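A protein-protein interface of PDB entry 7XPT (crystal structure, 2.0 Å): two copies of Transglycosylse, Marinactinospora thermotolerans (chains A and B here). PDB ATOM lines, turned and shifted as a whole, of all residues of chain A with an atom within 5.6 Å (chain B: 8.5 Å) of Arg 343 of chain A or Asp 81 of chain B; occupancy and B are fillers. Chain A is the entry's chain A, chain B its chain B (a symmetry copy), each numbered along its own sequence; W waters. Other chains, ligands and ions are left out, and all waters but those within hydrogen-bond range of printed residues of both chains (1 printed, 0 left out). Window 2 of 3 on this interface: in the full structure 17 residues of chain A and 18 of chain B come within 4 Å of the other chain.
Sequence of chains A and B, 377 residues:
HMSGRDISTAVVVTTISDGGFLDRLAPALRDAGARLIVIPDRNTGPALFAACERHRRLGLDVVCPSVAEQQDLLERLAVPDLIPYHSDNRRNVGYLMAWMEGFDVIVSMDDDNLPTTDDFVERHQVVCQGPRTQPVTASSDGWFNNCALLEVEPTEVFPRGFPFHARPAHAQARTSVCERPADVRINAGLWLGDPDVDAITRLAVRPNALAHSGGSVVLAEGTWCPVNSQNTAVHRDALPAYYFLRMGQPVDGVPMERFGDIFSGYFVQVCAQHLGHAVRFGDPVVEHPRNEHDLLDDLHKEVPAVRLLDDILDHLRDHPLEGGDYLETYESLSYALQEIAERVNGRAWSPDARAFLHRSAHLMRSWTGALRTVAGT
OE1 of Glu 342 of chain A lies within salt-bridge range of NH1 of Arg 246 of chain B, 3.95 Å away. NE of Arg 359 of chain B lies within salt-bridge range of OE2 of Glu 342 of chain A (2.7 Å). The backbone carbonyl oxygen of Glu 342 of chain A sits close to the side-chain carboxylate of Asp 81 of chain B (3.1 Å).
A ring nitrogen (NE2) of His 319 of chain A lies within hydrogen-bond range of the guanidinium group (NH1) of Arg 343 of chain A. The backbone carbonyl oxygen of Ala 341 of chain A sits at hydrogen-bond distance from the guanidinium group of Arg 354 of chain A, 2.7 Å away. The backbone carbonyl oxygen (O) of Val 344 of chain A lies within hydrogen-bond range of the guanidinium group (NH1) of Arg 354 of chain A, 2.8 Å away. The guanidinium group of Arg 354 of chain A sits at hydrogen-bond distance from the side-chain amide oxygen of Asn 345 of chain A (3.3 Å). The backbone carbonyl oxygen (O) of Asp 81 of chain B lies within hydrogen-bond range of the guanidinium group (NH1) of Arg 246 of chain B. The backbone carbonyl oxygen (O) of Leu 82 of chain B lies within hydrogen-bond range of the guanidinium group (NH1) of Arg 246 of chain B (3.4 Å).
Among the printed residues, merely in contact across the chains: Glu 339 of chain A with His 362 of chain B (3.9 Å), Glu 342 of chain A with His 362 of chain B (3.95 Å), Glu 342 of chain A with Leu 363 of chain B (3.9 Å), Arg 343 of chain A with Asp 81 of chain B (3.7 Å) and Arg 354 of chain A with Arg 359 of chain B (3.4 Å).
Arg 343 of chain A touches just one residue of chain B: Asp 81. Of chain A, only Glu 342 and Arg 343 come within 4 Å of Asp 81 of chain B. Printed residues of chain A within 4 Å of Arg 246 of chain B: Glu 342. Of the printed residues of chain B, Glu 339 of chain A touches His 362 (3.9 Å). The nearest printed residue of chain A that does not touch Arg 359 of chain B is Ala 341 of chain A (5.4 Å).
Of the 19 printed residues of chain B, 5 touch a printed residue of chain A. Printed residues of chain B that touch a printed residue of chain A: Asp 81, Arg 246, Arg 359, His 362 and Leu 363. Hydrophobic or aromatic side chains of chain B within 4 Å of the printed part of chain A: His 362 and Leu 363. Of the 10 printed residues of chain A, 4 touch a printed residue of chain B. Among the printed residues, 8 pairs touch across the chains. Among the printed residues, Asp or Glu carboxylates within 4 Å of a Lys or Arg side-chain nitrogen of the other chain: Glu 342 of chain A with Arg 246 of chain B (3.95 Å) and Glu 342 of chain A with Arg 359 of chain B (2.7 Å).
No position is printed for both chains. Of the 8 pairs that touch across the chains among the printed residues, none has its exchanged pair printed and touching as well.
Water W1 bridges O of Asp 81 of chain B and OE1 of Glu 342 of chain A.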
ATOM      1  N   HIS A 315     -35.306 -40.616   9.680  1.00  0.00           N
ATOM      2  CA  HIS A 315     -35.122 -39.181   9.855  1.00  0.00           C
ATOM      3  C   HIS A 315     -36.357 -38.498  10.425  1.00  0.00           C
ATOM      4  O   HIS A 315     -36.226 -37.437  11.043  1.00  0.00           O
ATOM      5  CB  HIS A 315     -34.732 -38.538   8.526  1.00  0.00           C
ATOM      6  CG  HIS A 315     -33.323 -38.821   8.111  1.00  0.00           C
ATOM      7  ND1 HIS A 315     -32.319 -37.883   8.203  1.00  0.00           N
ATOM      8  CD2 HIS A 315     -32.746 -39.941   7.610  1.00  0.00           C
ATOM      9  CE1 HIS A 315     -31.186 -38.409   7.774  1.00  0.00           C
ATOM     10  NE2 HIS A 315     -31.417 -39.657   7.409  1.00  0.00           N
ATOM     11  N   HIS A 319     -36.787 -35.362  13.618  1.00  0.00           N
ATOM     12  CA  HIS A 319     -37.241 -34.021  13.263  1.00  0.00           C
ATOM     13  C   HIS A 319     -38.484 -33.668  14.066  1.00  0.00           C
ATOM     14  O   HIS A 319     -39.589 -34.122  13.730  1.00  0.00           O
ATOM     15  CB  HIS A 319     -37.532 -33.930  11.763  1.00  0.00           C
ATOM     16  CG  HIS A 319     -36.391 -33.396  10.955  1.00  0.00           C
ATOM     17  ND1 HIS A 319     -36.276 -32.064  10.621  1.00  0.00           N
ATOM     18  CD2 HIS A 319     -35.318 -34.016  10.409  1.00  0.00           C
ATOM     19  CE1 HIS A 319     -35.179 -31.885   9.907  1.00  0.00           C
ATOM     20  NE2 HIS A 319     -34.580 -33.053   9.764  1.00  0.00           N
ATOM     21  N   GLU A 339     -35.780 -30.717   4.383  1.00  0.00           N
ATOM     22  CA  GLU A 339     -34.486 -30.825   5.051  1.00  0.00           C
ATOM     23  C   GLU A 339     -33.968 -32.255   5.006  1.00  0.00           C
ATOM     24  O   GLU A 339     -32.775 -32.482   4.778  1.00  0.00           O
ATOM     25  CB  GLU A 339     -34.592 -30.342   6.497  1.00  0.00           C
ATOM     26  CG  GLU A 339     -34.010 -28.958   6.739  1.00  0.00           C
ATOM     27  CD  GLU A 339     -34.792 -27.864   6.042  1.00  0.00           C
ATOM     28  OE1 GLU A 339     -35.997 -28.065   5.784  1.00  0.00           O
ATOM     29  OE2 GLU A 339     -34.202 -26.803   5.750  1.00  0.00           O
ATOM     30  N   ILE A 340     -34.852 -33.232   5.216  1.00  0.00           N
ATOM     31  CA  ILE A 340     -34.450 -34.634   5.173  1.00  0.00           C
ATOM     32  C   ILE A 340     -33.936 -35.001   3.785  1.00  0.00           C
ATOM     33  O   ILE A 340     -33.001 -35.799   3.643  1.00  0.00           O
ATOM     34  CB  ILE A 340     -35.626 -35.530   5.603  1.00  0.00           C
ATOM     35  CG1 ILE A 340     -35.943 -35.309   7.083  1.00  0.00           C
ATOM     36  CG2 ILE A 340     -35.321 -36.996   5.325  1.00  0.00           C
ATOM     37  CD1 ILE A 340     -37.212 -35.989   7.544  1.00  0.00           C
ATOM     38  N   ALA A 341     -34.523 -34.405   2.743  1.00  0.00           N
ATOM     39  CA  ALA A 341     -34.150 -34.743   1.373  1.00  0.00           C
ATOM     40  C   ALA A 341     -32.686 -34.436   1.085  1.00  0.00           C
ATOM     41  O   ALA A 341     -32.067 -35.107   0.250  1.00  0.00           O
ATOM     42  CB  ALA A 341     -35.051 -33.997   0.389  1.00  0.00           C
ATOM     43  N   GLU A 342     -32.113 -33.439   1.759  1.00  0.00           N
ATOM     44  CA  GLU A 342     -30.727 -33.062   1.519  1.00  0.00           C
ATOM     45  C   GLU A 342     -29.753 -33.656   2.526  1.00  0.00           C
ATOM     46  O   GLU A 342     -28.546 -33.664   2.261  1.00  0.00           O
ATOM     47  CB  GLU A 342     -30.582 -31.535   1.519  1.00  0.00           C
ATOM     48  CG  GLU A 342     -31.462 -30.833   0.496  1.00  0.00           C
ATOM     49  CD  GLU A 342     -31.160 -31.258  -0.928  1.00  0.00           C
ATOM     50  OE1 GLU A 342     -29.968 -31.415  -1.266  1.00  0.00           O
ATOM     51  OE2 GLU A 342     -32.117 -31.441  -1.708  1.00  0.00           O
ATOM     52  N   ARG A 343     -30.236 -34.150   3.665  1.00  0.00           N
ATOM     53  CA  ARG A 343     -29.355 -34.738   4.666  1.00  0.00           C
ATOM     54  C   ARG A 343     -29.166 -36.235   4.477  1.00  0.00           C
ATOM     55  O   ARG A 343     -28.081 -36.755   4.759  1.00  0.00           O
ATOM     56  CB  ARG A 343     -29.899 -34.485   6.075  1.00  0.00           C
ATOM     57  CG  ARG A 343     -30.115 -33.026   6.423  1.00  0.00           C
ATOM     58  CD  ARG A 343     -30.642 -32.891   7.844  1.00  0.00           C
ATOM     59  NE  ARG A 343     -31.143 -31.550   8.124  1.00  0.00           N
ATOM     60  CZ  ARG A 343     -31.612 -31.158   9.300  1.00  0.00           C
ATOM     61  NH1 ARG A 343     -31.642 -31.977  10.340  1.00  0.00           N
ATOM     62  NH2 ARG A 343     -32.061 -29.914   9.438  1.00  0.00           N
ATOM     63  N   VAL A 344     -30.197 -36.936   4.005  1.00  0.00           N
ATOM     64  CA  VAL A 344     -30.129 -38.387   3.901  1.00  0.00           C
ATOM     65  C   VAL A 344     -29.119 -38.789   2.831  1.00  0.00           C
ATOM     66  O   VAL A 344     -28.917 -38.088   1.828  1.00  0.00           O
ATOM     67  CB  VAL A 344     -31.526 -38.967   3.609  1.00  0.00           C
ATOM     68  CG1 VAL A 344     -32.003 -38.563   2.218  1.00  0.00           C
ATOM     69  CG2 VAL A 344     -31.528 -40.480   3.779  1.00  0.00           C
ATOM     70  N   ASN A 345     -28.457 -39.922   3.058  1.00  0.00           N
ATOM     71  CA  ASN A 345     -27.465 -40.457   2.139  1.00  0.00           C
ATOM     72  C   ASN A 345     -27.727 -41.936   1.897  1.00  0.00           C
ATOM     73  O   ASN A 345     -28.256 -42.641   2.760  1.00  0.00           O
ATOM     74  CB  ASN A 345     -26.041 -40.260   2.674  1.00  0.00           C
ATOM     75  CG  ASN A 345     -25.494 -38.879   2.374  1.00  0.00           C
ATOM     76  OD1 ASN A 345     -25.555 -38.408   1.237  1.00  0.00           O
ATOM     77  ND2 ASN A 345     -24.962 -38.219   3.396  1.00  0.00           N
ATOM     78  N   ARG A 354     -34.244 -37.365  -4.284  1.00  0.00           N
ATOM     79  CA  ARG A 354     -34.311 -36.224  -3.379  1.00  0.00           C
ATOM     80  C   ARG A 354     -35.375 -35.231  -3.827  1.00  0.00           C
ATOM     81  O   ARG A 354     -36.122 -34.697  -2.999  1.00  0.00           O
ATOM     82  CB  ARG A 354     -32.944 -35.546  -3.292  1.00  0.00           C
ATOM     83  CG  ARG A 354     -31.814 -36.472  -2.868  1.00  0.00           C
ATOM     84  CD  ARG A 354     -30.498 -35.720  -2.779  1.00  0.00           C
ATOM     85  NE  ARG A 354     -29.396 -36.585  -2.376  1.00  0.00           N
ATOM     86  CZ  ARG A 354     -29.036 -36.802  -1.119  1.00  0.00           C
ATOM     87  NH1 ARG A 354     -29.678 -36.236  -0.109  1.00  0.00           N
ATOM     88  NH2 ARG A 354     -28.005 -37.605  -0.867  1.00  0.00           N
ATOM     89  N   GLN B  71     -15.424 -26.371   3.545  1.00  0.00           N
ATOM     90  CA  GLN B  71     -16.460 -27.149   4.214  1.00  0.00           C
ATOM     91  C   GLN B  71     -16.680 -26.683   5.648  1.00  0.00           C
ATOM     92  O   GLN B  71     -17.801 -26.770   6.160  1.00  0.00           O
ATOM     93  CB  GLN B  71     -16.100 -28.634   4.185  1.00  0.00           C
ATOM     94  CG  GLN B  71     -17.209 -29.555   4.669  1.00  0.00           C
ATOM     95  CD  GLN B  71     -18.459 -29.471   3.810  1.00  0.00           C
ATOM     96  OE1 GLN B  71     -18.391 -29.144   2.624  1.00  0.00           O
ATOM     97  NE2 GLN B  71     -19.608 -29.761   4.409  1.00  0.00           N
ATOM     98  N   LEU B  74     -18.947 -23.627   5.372  1.00  0.00           N
ATOM     99  CA  LEU B  74     -20.299 -24.071   5.047  1.00  0.00           C
ATOM    100  C   LEU B  74     -20.950 -24.772   6.234  1.00  0.00           C
ATOM    101  O   LEU B  74     -22.152 -24.616   6.474  1.00  0.00           O
ATOM    102  CB  LEU B  74     -20.263 -24.988   3.823  1.00  0.00           C
ATOM    103  CG  LEU B  74     -19.709 -24.349   2.547  1.00  0.00           C
ATOM    104  CD1 LEU B  74     -19.346 -25.409   1.516  1.00  0.00           C
ATOM    105  CD2 LEU B  74     -20.708 -23.356   1.968  1.00  0.00           C
ATOM    106  N   GLU B  75     -20.167 -25.546   6.989  1.00  0.00           N
ATOM    107  CA  GLU B  75     -20.687 -26.182   8.197  1.00  0.00           C
ATOM    108  C   GLU B  75     -21.174 -25.147   9.203  1.00  0.00           C
ATOM    109  O   GLU B  75     -22.244 -25.310   9.803  1.00  0.00           O
ATOM    110  CB  GLU B  75     -19.611 -27.069   8.826  1.00  0.00           C
ATOM    111  CG  GLU B  75     -19.784 -28.549   8.553  1.00  0.00           C
ATOM    112  CD  GLU B  75     -20.883 -29.169   9.392  1.00  0.00           C
ATOM    113  OE1 GLU B  75     -21.056 -28.743  10.554  1.00  0.00           O
ATOM    114  OE2 GLU B  75     -21.576 -30.079   8.890  1.00  0.00           O
ATOM    115  N   ALA B  78     -24.618 -23.729   8.523  1.00  0.00           N
ATOM    116  CA  ALA B  78     -25.709 -24.704   8.505  1.00  0.00           C
ATOM    117  C   ALA B  78     -26.111 -25.092   7.084  1.00  0.00           C
ATOM    118  O   ALA B  78     -27.279 -25.374   6.815  1.00  0.00           O
ATOM    119  CB  ALA B  78     -26.925 -24.196   9.286  1.00  0.00           C
ATOM    120  N   VAL B  79     -25.149 -25.114   6.164  1.00  0.00           N
ATOM    121  CA  VAL B  79     -25.404 -25.568   4.797  1.00  0.00           C
ATOM    122  C   VAL B  79     -24.317 -26.545   4.356  1.00  0.00           C
ATOM    123  O   VAL B  79     -23.665 -26.313   3.326  1.00  0.00           O
ATOM    124  CB  VAL B  79     -25.503 -24.381   3.826  1.00  0.00           C
ATOM    125  CG1 VAL B  79     -26.867 -23.719   3.933  1.00  0.00           C
ATOM    126  CG2 VAL B  79     -24.399 -23.366   4.105  1.00  0.00           C
ATOM    127  N   PRO B  80     -24.094 -27.653   5.072  1.00  0.00           N
ATOM    128  CA  PRO B  80     -22.997 -28.553   4.687  1.00  0.00           C
ATOM    129  C   PRO B  80     -23.269 -29.345   3.420  1.00  0.00           C
ATOM    130  O   PRO B  80     -22.311 -29.787   2.773  1.00  0.00           O
ATOM    131  CB  PRO B  80     -22.865 -29.478   5.903  1.00  0.00           C
ATOM    132  CG  PRO B  80     -24.244 -29.539   6.457  1.00  0.00           C
ATOM    133  CD  PRO B  80     -24.856 -28.179   6.221  1.00  0.00           C
ATOM    134  N   ASP B  81     -24.533 -29.534   3.041  1.00  0.00           N
ATOM    135  CA  ASP B  81     -24.894 -30.327   1.874  1.00  0.00           C
ATOM    136  C   ASP B  81     -25.289 -29.469   0.677  1.00  0.00           C
ATOM    137  O   ASP B  81     -25.736 -30.014  -0.338  1.00  0.00           O
ATOM    138  CB  ASP B  81     -26.038 -31.280   2.221  1.00  0.00           C
ATOM    139  CG  ASP B  81     -25.748 -32.114   3.453  1.00  0.00           C
ATOM    140  OD1 ASP B  81     -24.604 -32.596   3.592  1.00  0.00           O
ATOM    141  OD2 ASP B  81     -26.665 -32.282   4.285  1.00  0.00           O
ATOM    142  N   LEU B  82     -25.131 -28.149   0.770  1.00  0.00           N
ATOM    143  CA  LEU B  82     -25.624 -27.269  -0.285  1.00  0.00           C
ATOM    144  C   LEU B  82     -24.775 -27.377  -1.545  1.00  0.00           C
ATOM    145  O   LEU B  82     -25.307 -27.502  -2.656  1.00  0.00           O
ATOM    146  CB  LEU B  82     -25.662 -25.824   0.212  1.00  0.00           C
ATOM    147  CG  LEU B  82     -26.034 -24.760  -0.824  1.00  0.00           C
ATOM    148  CD1 LEU B  82     -27.394 -25.056  -1.444  1.00  0.00           C
ATOM    149  CD2 LEU B  82     -26.013 -23.368  -0.203  1.00  0.00           C
ATOM    150  N   ILE B  83     -23.459 -27.327  -1.398  1.00  0.00           N
ATOM    151  CA  ILE B  83     -22.531 -27.237  -2.521  1.00  0.00           C
ATOM    152  C   ILE B  83     -21.840 -28.586  -2.681  1.00  0.00           C
ATOM    153  O   ILE B  83     -21.137 -29.029  -1.761  1.00  0.00           O
ATOM    154  CB  ILE B  83     -21.510 -26.106  -2.315  1.00  0.00           C
ATOM    155  CG1 ILE B  83     -22.246 -24.769  -2.182  1.00  0.00           C
ATOM    156  CG2 ILE B  83     -20.519 -26.067  -3.462  1.00  0.00           C
ATOM    157  CD1 ILE B  83     -21.354 -23.600  -1.878  1.00  0.00           C
ATOM    158  N   PRO B  84     -22.007 -29.270  -3.807  1.00  0.00           N
ATOM    159  CA  PRO B  84     -21.378 -30.582  -3.988  1.00  0.00           C
ATOM    160  C   PRO B  84     -19.926 -30.452  -4.432  1.00  0.00           C
ATOM    161  O   PRO B  84     -19.447 -29.385  -4.816  1.00  0.00           O
ATOM    162  CB  PRO B  84     -22.233 -31.223  -5.082  1.00  0.00           C
ATOM    163  CG  PRO B  84     -22.669 -30.059  -5.912  1.00  0.00           C
ATOM    164  CD  PRO B  84     -22.867 -28.909  -4.949  1.00  0.00           C
ATOM    165  N   TYR B  85     -19.226 -31.578  -4.383  1.00  0.00           N
ATOM    166  CA  TYR B  85     -17.849 -31.656  -4.840  1.00  0.00           C
ATOM    167  C   TYR B  85     -17.792 -32.222  -6.255  1.00  0.00           C
ATOM    168  O   TYR B  85     -18.781 -32.727  -6.791  1.00  0.00           O
ATOM    169  CB  TYR B  85     -17.012 -32.499  -3.873  1.00  0.00           C
ATOM    170  CG  TYR B  85     -16.833 -31.835  -2.525  1.00  0.00           C
ATOM    171  CD1 TYR B  85     -15.826 -30.902  -2.319  1.00  0.00           C
ATOM    172  CD2 TYR B  85     -17.679 -32.132  -1.464  1.00  0.00           C
ATOM    173  CE1 TYR B  85     -15.659 -30.288  -1.092  1.00  0.00           C
ATOM    174  CE2 TYR B  85     -17.520 -31.521  -0.233  1.00  0.00           C
ATOM    175  CZ  TYR B  85     -16.509 -30.599  -0.053  1.00  0.00           C
ATOM    176  OH  TYR B  85     -16.345 -29.988   1.169  1.00  0.00           O
ATOM    177  N   ASN B  89     -19.976 -25.968  -9.461  1.00  0.00           N
ATOM    178  CA  ASN B  89     -20.900 -25.294  -8.557  1.00  0.00           C
ATOM    179  C   ASN B  89     -20.182 -24.706  -7.349  1.00  0.00           C
ATOM    180  O   ASN B  89     -20.734 -23.828  -6.675  1.00  0.00           O
ATOM    181  CB  ASN B  89     -21.987 -26.272  -8.102  1.00  0.00           C
ATOM    182  CG  ASN B  89     -23.144 -25.583  -7.403  1.00  0.00           C
ATOM    183  OD1 ASN B  89     -23.182 -25.501  -6.176  1.00  0.00           O
ATOM    184  ND2 ASN B  89     -24.101 -25.096  -8.184  1.00  0.00           N
ATOM    185  N   ARG B  90     -18.957 -25.162  -7.070  1.00  0.00           N
ATOM    186  CA  ARG B  90     -18.191 -24.670  -5.933  1.00  0.00           C
ATOM    187  C   ARG B  90     -17.788 -23.207  -6.073  1.00  0.00           C
ATOM    188  O   ARG B  90     -17.267 -22.636  -5.110  1.00  0.00           O
ATOM    189  CB  ARG B  90     -16.942 -25.527  -5.725  1.00  0.00           C
ATOM    190  CG  ARG B  90     -17.242 -26.992  -5.467  1.00  0.00           C
ATOM    191  CD  ARG B  90     -16.173 -27.627  -4.599  1.00  0.00           C
ATOM    192  NE  ARG B  90     -16.137 -27.032  -3.268  1.00  0.00           N
ATOM    193  CZ  ARG B  90     -16.936 -27.381  -2.270  1.00  0.00           C
ATOM    194  NH1 ARG B  90     -17.855 -28.322  -2.416  1.00  0.00           N
ATOM    195  NH2 ARG B  90     -16.811 -26.772  -1.095  1.00  0.00           N
ATOM    196  N   TYR B 243     -26.834 -16.976  -7.153  1.00  0.00           N
ATOM    197  CA  TYR B 243     -26.466 -18.337  -6.787  1.00  0.00           C
ATOM    198  C   TYR B 243     -26.424 -19.237  -8.018  1.00  0.00           C
ATOM    199  O   TYR B 243     -27.369 -19.272  -8.811  1.00  0.00           O
ATOM    200  CB  TYR B 243     -27.457 -18.872  -5.752  1.00  0.00           C
ATOM    201  CG  TYR B 243     -27.556 -20.376  -5.672  1.00  0.00           C
ATOM    202  CD1 TYR B 243     -26.549 -21.129  -5.087  1.00  0.00           C
ATOM    203  CD2 TYR B 243     -28.675 -21.040  -6.155  1.00  0.00           C
ATOM    204  CE1 TYR B 243     -26.644 -22.504  -5.001  1.00  0.00           C
ATOM    205  CE2 TYR B 243     -28.781 -22.413  -6.076  1.00  0.00           C
ATOM    206  CZ  TYR B 243     -27.764 -23.139  -5.498  1.00  0.00           C
ATOM    207  OH  TYR B 243     -27.864 -24.507  -5.415  1.00  0.00           O
ATOM    208  N   ARG B 246     -27.558 -25.670  -8.936  1.00  0.00           N
ATOM    209  CA  ARG B 246     -27.002 -27.014  -8.885  1.00  0.00           C
ATOM    210  C   ARG B 246     -27.543 -27.854 -10.038  1.00  0.00           C
ATOM    211  O   ARG B 246     -28.754 -27.902 -10.271  1.00  0.00           O
ATOM    212  CB  ARG B 246     -27.340 -27.662  -7.544  1.00  0.00           C
ATOM    213  CG  ARG B 246     -26.679 -28.999  -7.293  1.00  0.00           C
ATOM    214  CD  ARG B 246     -26.884 -29.410  -5.845  1.00  0.00           C
ATOM    215  NE  ARG B 246     -26.297 -30.708  -5.543  1.00  0.00           N
ATOM    216  CZ  ARG B 246     -26.220 -31.224  -4.326  1.00  0.00           C
ATOM    217  NH1 ARG B 246     -26.667 -30.567  -3.268  1.00  0.00           N
ATOM    218  NH2 ARG B 246     -25.680 -32.429  -4.163  1.00  0.00           N
ATOM    219  N   ARG B 359     -36.765 -28.820  -6.165  1.00  0.00           N
ATOM    220  CA  ARG B 359     -35.509 -28.950  -5.433  1.00  0.00           C
ATOM    221  C   ARG B 359     -34.599 -27.752  -5.675  1.00  0.00           C
ATOM    222  O   ARG B 359     -33.868 -27.340  -4.767  1.00  0.00           O
ATOM    223  CB  ARG B 359     -34.795 -30.247  -5.815  1.00  0.00           C
ATOM    224  CG  ARG B 359     -33.461 -30.445  -5.103  1.00  0.00           C
ATOM    225  CD  ARG B 359     -33.017 -31.900  -5.111  1.00  0.00           C
ATOM    226  NE  ARG B 359     -31.852 -32.120  -4.259  1.00  0.00           N
ATOM    227  CZ  ARG B 359     -30.636 -32.413  -4.701  1.00  0.00           C
ATOM    228  NH1 ARG B 359     -30.385 -32.553  -5.993  1.00  0.00           N
ATOM    229  NH2 ARG B 359     -29.649 -32.577  -3.825  1.00  0.00           N
ATOM    230  N   HIS B 362     -35.702 -25.024  -3.292  1.00  0.00           N
ATOM    231  CA  HIS B 362     -35.237 -25.252  -1.928  1.00  0.00           C
ATOM    232  C   HIS B 362     -33.774 -24.853  -1.778  1.00  0.00           C
ATOM    233  O   HIS B 362     -33.399 -24.182  -0.808  1.00  0.00           O
ATOM    234  CB  HIS B 362     -35.437 -26.716  -1.539  1.00  0.00           C
ATOM    235  CG  HIS B 362     -34.853 -27.070  -0.206  1.00  0.00           C
ATOM    236  ND1 HIS B 362     -35.570 -26.982   0.968  1.00  0.00           N
ATOM    237  CD2 HIS B 362     -33.619 -27.507   0.139  1.00  0.00           C
ATOM    238  CE1 HIS B 362     -34.803 -27.352   1.978  1.00  0.00           C
ATOM    239  NE2 HIS B 362     -33.615 -27.676   1.502  1.00  0.00           N
ATOM    240  N   LEU B 363     -32.931 -25.261  -2.731  1.00  0.00           N
ATOM    241  CA  LEU B 363     -31.520 -24.903  -2.675  1.00  0.00           C
ATOM    242  C   LEU B 363     -31.322 -23.400  -2.798  1.00  0.00           C
ATOM    243  O   LEU B 363     -30.386 -22.847  -2.213  1.00  0.00           O
ATOM    244  CB  LEU B 363     -30.749 -25.635  -3.774  1.00  0.00           C
ATOM    245  CG  LEU B 363     -30.779 -27.164  -3.704  1.00  0.00           C
ATOM    246  CD1 LEU B 363     -30.074 -27.770  -4.907  1.00  0.00           C
ATOM    247  CD2 LEU B 363     -30.158 -27.660  -2.405  1.00  0.00           C
ATOM    248  N   SER B 366     -32.072 -22.266   0.627  1.00  0.00           N
ATOM    249  CA  SER B 366     -30.955 -22.667   1.473  1.00  0.00           C
ATOM    250  C   SER B 366     -29.766 -21.735   1.289  1.00  0.00           C
ATOM    251  O   SER B 366     -29.027 -21.474   2.247  1.00  0.00           O
ATOM    252  CB  SER B 366     -30.557 -24.111   1.160  1.00  0.00           C
ATOM    253  OG  SER B 366     -29.462 -24.530   1.955  1.00  0.00           O
HETATM  254  O   HOH W   1     -28.275 -29.533  -0.271  1.00  0.00           O
